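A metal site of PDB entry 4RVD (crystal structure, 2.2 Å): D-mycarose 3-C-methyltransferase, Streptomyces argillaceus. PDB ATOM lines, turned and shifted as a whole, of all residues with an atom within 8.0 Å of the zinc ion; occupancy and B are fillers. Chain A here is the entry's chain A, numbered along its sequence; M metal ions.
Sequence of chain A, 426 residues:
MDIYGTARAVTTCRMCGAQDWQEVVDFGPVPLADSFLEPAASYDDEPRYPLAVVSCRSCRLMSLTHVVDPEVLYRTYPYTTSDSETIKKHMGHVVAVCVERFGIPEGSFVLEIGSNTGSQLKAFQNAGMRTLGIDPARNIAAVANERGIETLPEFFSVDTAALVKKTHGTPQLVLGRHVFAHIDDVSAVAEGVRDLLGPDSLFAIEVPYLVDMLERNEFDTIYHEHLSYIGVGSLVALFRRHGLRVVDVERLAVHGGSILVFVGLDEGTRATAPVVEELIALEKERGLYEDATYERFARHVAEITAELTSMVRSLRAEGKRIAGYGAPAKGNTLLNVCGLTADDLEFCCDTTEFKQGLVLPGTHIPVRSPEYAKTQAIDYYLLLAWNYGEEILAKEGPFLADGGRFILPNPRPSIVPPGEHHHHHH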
ATOM      1  N   THR A  12     -26.370  -9.061 -14.570  1.00  0.00           N
ATOM      2  CA  THR A  12     -25.908  -7.732 -14.882  1.00  0.00           C
ATOM      3  C   THR A  12     -25.662  -7.535 -16.396  1.00  0.00           C
ATOM      4  O   THR A  12     -25.396  -8.483 -17.134  1.00  0.00           O
ATOM      5  CB  THR A  12     -24.637  -7.380 -14.072  1.00  0.00           C
ATOM      6  OG1 THR A  12     -24.428  -5.970 -14.119  1.00  0.00           O
ATOM      7  CG2 THR A  12     -23.406  -8.108 -14.594  1.00  0.00           C
ATOM      8  N   CYS A  13     -25.761  -6.277 -16.811  1.00  0.00           N
ATOM      9  CA  CYS A  13     -25.599  -5.876 -18.204  1.00  0.00           C
ATOM     10  C   CYS A  13     -24.152  -5.971 -18.710  1.00  0.00           C
ATOM     11  O   CYS A  13     -23.224  -5.477 -18.059  1.00  0.00           O
ATOM     12  CB  CYS A  13     -26.103  -4.433 -18.349  1.00  0.00           C
ATOM     13  SG  CYS A  13     -25.714  -3.667 -19.929  1.00  0.00           S
ATOM     14  N   ARG A  14     -23.979  -6.609 -19.862  1.00  0.00           N
ATOM     15  CA  ARG A  14     -22.659  -6.822 -20.499  1.00  0.00           C
ATOM     16  C   ARG A  14     -21.877  -5.548 -20.764  1.00  0.00           C
ATOM     17  O   ARG A  14     -20.647  -5.543 -20.696  1.00  0.00           O
ATOM     18  CB  ARG A  14     -22.830  -7.497 -21.864  1.00  0.00           C
ATOM     19  CG  ARG A  14     -23.212  -8.962 -21.828  1.00  0.00           C
ATOM     20  CD  ARG A  14     -23.340  -9.506 -23.239  1.00  0.00           C
ATOM     21  NE  ARG A  14     -24.735  -9.540 -23.680  1.00  0.00           N
ATOM     22  CZ  ARG A  14     -25.608 -10.491 -23.360  1.00  0.00           C
ATOM     23  NH1 ARG A  14     -25.274 -11.509 -22.575  1.00  0.00           N
ATOM     24  NH2 ARG A  14     -26.837 -10.420 -23.830  1.00  0.00           N
ATOM     25  N   MET A  15     -22.580  -4.484 -21.146  1.00  0.00           N
ATOM     26  CA  MET A  15     -21.931  -3.273 -21.635  1.00  0.00           C
ATOM     27  C   MET A  15     -21.596  -2.277 -20.514  1.00  0.00           C
ATOM     28  O   MET A  15     -20.455  -1.819 -20.428  1.00  0.00           O
ATOM     29  CB  MET A  15     -22.817  -2.591 -22.687  1.00  0.00           C
ATOM     30  CG  MET A  15     -23.142  -3.474 -23.897  1.00  0.00           C
ATOM     31  SD  MET A  15     -21.756  -3.687 -25.039  1.00  0.00           S
ATOM     32  CE  MET A  15     -22.418  -4.920 -26.152  1.00  0.00           C
ATOM     33  N   CYS A  16     -22.583  -1.942 -19.667  1.00  0.00           N
ATOM     34  CA  CYS A  16     -22.403  -0.909 -18.627  1.00  0.00           C
ATOM     35  C   CYS A  16     -22.365  -1.432 -17.189  1.00  0.00           C
ATOM     36  O   CYS A  16     -21.903  -0.721 -16.296  1.00  0.00           O
ATOM     37  CB  CYS A  16     -23.482   0.168 -18.756  1.00  0.00           C
ATOM     38  SG  CYS A  16     -25.105  -0.324 -18.125  1.00  0.00           S
ATOM     39  N   GLY A  17     -22.837  -2.644 -16.962  1.00  0.00           N
ATOM     40  CA  GLY A  17     -22.745  -3.282 -15.642  1.00  0.00           C
ATOM     41  C   GLY A  17     -23.903  -3.013 -14.684  1.00  0.00           C
ATOM     42  O   GLY A  17     -23.881  -3.478 -13.552  1.00  0.00           O
ATOM     43  N   ALA A  18     -24.909  -2.280 -15.140  1.00  0.00           N
ATOM     44  CA  ALA A  18     -26.100  -2.018 -14.338  1.00  0.00           C
ATOM     45  C   ALA A  18     -27.035  -3.222 -14.341  1.00  0.00           C
ATOM     46  O   ALA A  18     -26.763  -4.234 -14.976  1.00  0.00           O
ATOM     47  CB  ALA A  18     -26.821  -0.787 -14.847  1.00  0.00           C
ATOM     48  N   GLN A  19     -28.140  -3.109 -13.612  1.00  0.00           N
ATOM     49  CA  GLN A  19     -29.156  -4.158 -13.575  1.00  0.00           C
ATOM     50  C   GLN A  19     -30.534  -3.505 -13.437  1.00  0.00           C
ATOM     51  O   GLN A  19     -31.146  -3.531 -12.386  1.00  0.00           O
ATOM     52  CB  GLN A  19     -28.866  -5.133 -12.435  1.00  0.00           C
ATOM     53  CG  GLN A  19     -29.778  -6.359 -12.401  1.00  0.00           C
ATOM     54  CD  GLN A  19     -29.224  -7.504 -11.574  1.00  0.00           C
ATOM     55  OE1 GLN A  19     -28.162  -7.391 -10.954  1.00  0.00           O
ATOM     56  NE2 GLN A  19     -29.937  -8.622 -11.567  1.00  0.00           N
ATOM     57  N   ASP A  20     -30.977  -2.903 -14.538  1.00  0.00           N
ATOM     58  CA  ASP A  20     -32.297  -2.272 -14.606  1.00  0.00           C
ATOM     59  C   ASP A  20     -32.905  -2.643 -15.954  1.00  0.00           C
ATOM     60  O   ASP A  20     -32.826  -1.887 -16.926  1.00  0.00           O
ATOM     61  CB  ASP A  20     -32.156  -0.756 -14.440  1.00  0.00           C
ATOM     62  CG  ASP A  20     -33.506  -0.031 -14.352  1.00  0.00           C
ATOM     63  OD1 ASP A  20     -33.500   1.203 -14.216  1.00  0.00           O
ATOM     64  OD2 ASP A  20     -34.561  -0.694 -14.447  1.00  0.00           O
ATOM     65  N   TRP A  21     -33.519  -3.829 -15.995  1.00  0.00           N
ATOM     66  CA  TRP A  21     -34.033  -4.426 -17.230  1.00  0.00           C
ATOM     67  C   TRP A  21     -35.522  -4.163 -17.450  1.00  0.00           C
ATOM     68  O   TRP A  21     -36.344  -4.501 -16.606  1.00  0.00           O
ATOM     69  CB  TRP A  21     -33.817  -5.939 -17.185  1.00  0.00           C
ATOM     70  CG  TRP A  21     -32.384  -6.381 -17.139  1.00  0.00           C
ATOM     71  CD1 TRP A  21     -31.741  -6.980 -16.091  1.00  0.00           C
ATOM     72  CD2 TRP A  21     -31.406  -6.271 -18.189  1.00  0.00           C
ATOM     73  NE1 TRP A  21     -30.436  -7.245 -16.425  1.00  0.00           N
ATOM     74  CE2 TRP A  21     -30.205  -6.827 -17.701  1.00  0.00           C
ATOM     75  CE3 TRP A  21     -31.440  -5.757 -19.495  1.00  0.00           C
ATOM     76  CZ2 TRP A  21     -29.043  -6.885 -18.475  1.00  0.00           C
ATOM     77  CZ3 TRP A  21     -30.289  -5.822 -20.256  1.00  0.00           C
ATOM     78  CH2 TRP A  21     -29.103  -6.373 -19.744  1.00  0.00           C
ATOM     79  N   SER A  55     -34.267  -4.859 -22.132  1.00  0.00           N
ATOM     80  CA  SER A  55     -33.575  -3.624 -22.489  1.00  0.00           C
ATOM     81  C   SER A  55     -33.000  -2.956 -21.239  1.00  0.00           C
ATOM     82  O   SER A  55     -33.708  -2.752 -20.260  1.00  0.00           O
ATOM     83  CB  SER A  55     -34.541  -2.655 -23.179  1.00  0.00           C
ATOM     84  OG  SER A  55     -33.917  -1.410 -23.470  1.00  0.00           O
ATOM     85  N   CYS A  56     -31.717  -2.615 -21.301  1.00  0.00           N
ATOM     86  CA  CYS A  56     -31.038  -1.991 -20.163  1.00  0.00           C
ATOM     87  C   CYS A  56     -31.343  -0.491 -20.117  1.00  0.00           C
ATOM     88  O   CYS A  56     -31.024   0.236 -21.057  1.00  0.00           O
ATOM     89  CB  CYS A  56     -29.531  -2.226 -20.255  1.00  0.00           C
ATOM     90  SG  CYS A  56     -28.517  -1.262 -19.102  1.00  0.00           S
ATOM     91  N   ARG A  57     -31.956  -0.020 -19.027  1.00  0.00           N
ATOM     92  CA  ARG A  57     -32.330   1.398 -18.912  1.00  0.00           C
ATOM     93  C   ARG A  57     -31.146   2.358 -18.735  1.00  0.00           C
ATOM     94  O   ARG A  57     -31.276   3.552 -19.019  1.00  0.00           O
ATOM     95  CB  ARG A  57     -33.343   1.600 -17.777  1.00  0.00           C
ATOM     96  CG  ARG A  57     -34.691   0.955 -18.046  1.00  0.00           C
ATOM     97  CD  ARG A  57     -35.805   1.651 -17.270  1.00  0.00           C
ATOM     98  NE  ARG A  57     -37.117   1.097 -17.571  1.00  0.00           N
ATOM     99  CZ  ARG A  57     -37.619  -0.018 -17.035  1.00  0.00           C
ATOM    100  NH1 ARG A  57     -36.923  -0.727 -16.167  1.00  0.00           N
ATOM    101  NH2 ARG A  57     -38.832  -0.422 -17.385  1.00  0.00           N
ATOM    102  N   SER A  58     -30.004   1.842 -18.277  1.00  0.00           N
ATOM    103  CA  SER A  58     -28.791   2.676 -18.172  1.00  0.00           C
ATOM    104  C   SER A  58     -28.213   3.050 -19.549  1.00  0.00           C
ATOM    105  O   SER A  58     -28.196   4.225 -19.914  1.00  0.00           O
ATOM    106  CB  SER A  58     -27.733   1.968 -17.329  1.00  0.00           C
ATOM    107  OG  SER A  58     -26.473   2.617 -17.451  1.00  0.00           O
ATOM    108  N   CYS A  59     -27.775   2.042 -20.301  1.00  0.00           N
ATOM    109  CA  CYS A  59     -27.092   2.248 -21.580  1.00  0.00           C
ATOM    110  C   CYS A  59     -27.936   1.896 -22.818  1.00  0.00           C
ATOM    111  O   CYS A  59     -27.580   2.261 -23.933  1.00  0.00           O
ATOM    112  CB  CYS A  59     -25.796   1.427 -21.611  1.00  0.00           C
ATOM    113  SG  CYS A  59     -26.057  -0.348 -21.862  1.00  0.00           S
ATOM    114  N   ARG A  60     -29.029   1.159 -22.594  1.00  0.00           N
ATOM    115  CA  ARG A  60     -29.968   0.733 -23.645  1.00  0.00           C
ATOM    116  C   ARG A  60     -29.391  -0.295 -24.619  1.00  0.00           C
ATOM    117  O   ARG A  60     -29.764  -0.352 -25.786  1.00  0.00           O
ATOM    118  CB  ARG A  60     -30.614   1.928 -24.362  1.00  0.00           C
ATOM    119  CG  ARG A  60     -31.624   2.680 -23.499  1.00  0.00           C
ATOM    120  CD  ARG A  60     -32.868   1.841 -23.177  1.00  0.00           C
ATOM    121  NE  ARG A  60     -33.882   2.603 -22.446  1.00  0.00           N
ATOM    122  CZ  ARG A  60     -35.042   2.115 -22.015  1.00  0.00           C
ATOM    123  NH1 ARG A  60     -35.367   0.840 -22.235  1.00  0.00           N
ATOM    124  NH2 ARG A  60     -35.886   2.904 -21.362  1.00  0.00           N
ATOM    125  N   LEU A  61     -28.504  -1.140 -24.102  1.00  0.00           N
ATOM    126  CA  LEU A  61     -28.259  -2.431 -24.698  1.00  0.00           C
ATOM    127  C   LEU A  61     -29.559  -3.199 -24.634  1.00  0.00           C
ATOM    128  O   LEU A  61     -30.259  -3.168 -23.618  1.00  0.00           O
ATOM    129  CB  LEU A  61     -27.186  -3.222 -23.946  1.00  0.00           C
ATOM    130  CG  LEU A  61     -27.093  -4.717 -24.327  1.00  0.00           C
ATOM    131  CD1 LEU A  61     -26.627  -4.849 -25.769  1.00  0.00           C
ATOM    132  CD2 LEU A  61     -26.187  -5.495 -23.377  1.00  0.00           C
ATOM    133  N   MET A  62     -29.884  -3.867 -25.732  1.00  0.00           N
ATOM    134  CA  MET A  62     -30.948  -4.836 -25.718  1.00  0.00           C
ATOM    135  C   MET A  62     -30.283  -6.211 -25.682  1.00  0.00           C
ATOM    136  O   MET A  62     -29.373  -6.491 -26.455  1.00  0.00           O
ATOM    137  CB  MET A  62     -31.822  -4.623 -26.935  1.00  0.00           C
ATOM    138  CG  MET A  62     -33.117  -5.409 -26.932  1.00  0.00           C
ATOM    139  SD  MET A  62     -34.360  -4.593 -27.936  1.00  0.00           S
ATOM    140  CE  MET A  62     -35.071  -6.024 -28.753  1.00  0.00           C
ATOM    141  N   SER A 234     -24.577   2.149 -26.269  1.00  0.00           N
ATOM    142  CA  SER A 234     -24.114   1.070 -25.396  1.00  0.00           C
ATOM    143  C   SER A 234     -22.653   0.687 -25.646  1.00  0.00           C
ATOM    144  O   SER A 234     -21.971   0.222 -24.724  1.00  0.00           O
ATOM    145  CB  SER A 234     -25.011  -0.165 -25.539  1.00  0.00           C
ATOM    146  OG  SER A 234     -24.991  -0.702 -26.848  1.00  0.00           O
ATOM    147  N   ALA A 237     -20.575   3.214 -23.745  1.00  0.00           N
ATOM    148  CA  ALA A 237     -20.628   2.844 -22.316  1.00  0.00           C
ATOM    149  C   ALA A 237     -19.641   1.734 -21.981  1.00  0.00           C
ATOM    150  O   ALA A 237     -19.001   1.774 -20.921  1.00  0.00           O
ATOM    151  CB  ALA A 237     -22.028   2.436 -21.920  1.00  0.00           C
ATOM    152  N   LEU A 238     -19.528   0.735 -22.849  1.00  0.00           N
ATOM    153  CA  LEU A 238     -18.590  -0.363 -22.617  1.00  0.00           C
ATOM    154  C   LEU A 238     -17.145   0.101 -22.749  1.00  0.00           C
ATOM    155  O   LEU A 238     -16.341  -0.104 -21.835  1.00  0.00           O
ATOM    156  CB  LEU A 238     -18.807  -1.497 -23.614  1.00  0.00           C
ATOM    157  CG  LEU A 238     -17.671  -2.514 -23.591  1.00  0.00           C
ATOM    158  CD1 LEU A 238     -17.813  -3.452 -22.403  1.00  0.00           C
ATOM    159  CD2 LEU A 238     -17.622  -3.264 -24.918  1.00  0.00           C
ATOM    160  N   ARG A 241     -14.949   2.124 -20.237  1.00  0.00           N
ATOM    161  CA  ARG A 241     -14.466   1.440 -19.049  1.00  0.00           C
ATOM    162  C   ARG A 241     -13.262   0.547 -19.302  1.00  0.00           C
ATOM    163  O   ARG A 241     -12.867  -0.208 -18.419  1.00  0.00           O
ATOM    164  CB  ARG A 241     -15.597   0.590 -18.464  1.00  0.00           C
ATOM    165  CG  ARG A 241     -16.885   1.347 -18.207  1.00  0.00           C
ATOM    166  CD  ARG A 241     -17.814   0.544 -17.299  1.00  0.00           C
ATOM    167  NE  ARG A 241     -18.166  -0.758 -17.880  1.00  0.00           N
ATOM    168  CZ  ARG A 241     -18.680  -1.785 -17.192  1.00  0.00           C
ATOM    169  NH1 ARG A 241     -18.907  -1.686 -15.881  1.00  0.00           N
ATOM    170  NH2 ARG A 241     -18.957  -2.913 -17.818  1.00  0.00           N
HETATM  171 ZN    ZN M   1     -26.310  -1.419 -19.816  1.00  0.00          ZN
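Four residues have an atom within 4 Å of the zinc ion: Cys 13, Cys 16, Cys 56 and Cys 59.
The zinc ion is bound by the side-chain sulfur (SG) of Cys 59 (2.3 Å), the side-chain sulfur (SG) of Cys 56 (2.3 Å), the side-chain sulfur (SG) of Cys 13 (2.3 Å) and the side-chain sulfur (SG) of Cys 16 (2.3 Å).
The side-chain sulfur (SG) of Cys 13 lies close to the backbone NH (N) of Met 15 (3.5 Å).
The backbone NH (N) of Cys 13 is in hydrogen-bond range of the backbone carbonyl oxygen (O) of Ala 18, 2.9 Å away.
The side-chain sulfur of Cys 16 sits close to the side-chain hydroxyl of Ser 58.
The side-chain sulfur (SG) of Cys 59 sits close to the backbone NH (N) of Leu 61 (3.4 Å).
SG of Cys 56 lies close to N of Ser 58 (3.5 Å).
O of Cys 16 lies within hydrogen-bond range of NH1 of Arg 241 (3.2 Å).
The backbone carbonyl oxygen (O) of Leu 61 sits at hydrogen-bond distance from the backbone NH (N) of Cys 56, at 2.8 Å.
SG of Cys 16 sits close to N of Ala 18 (3.6 Å).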
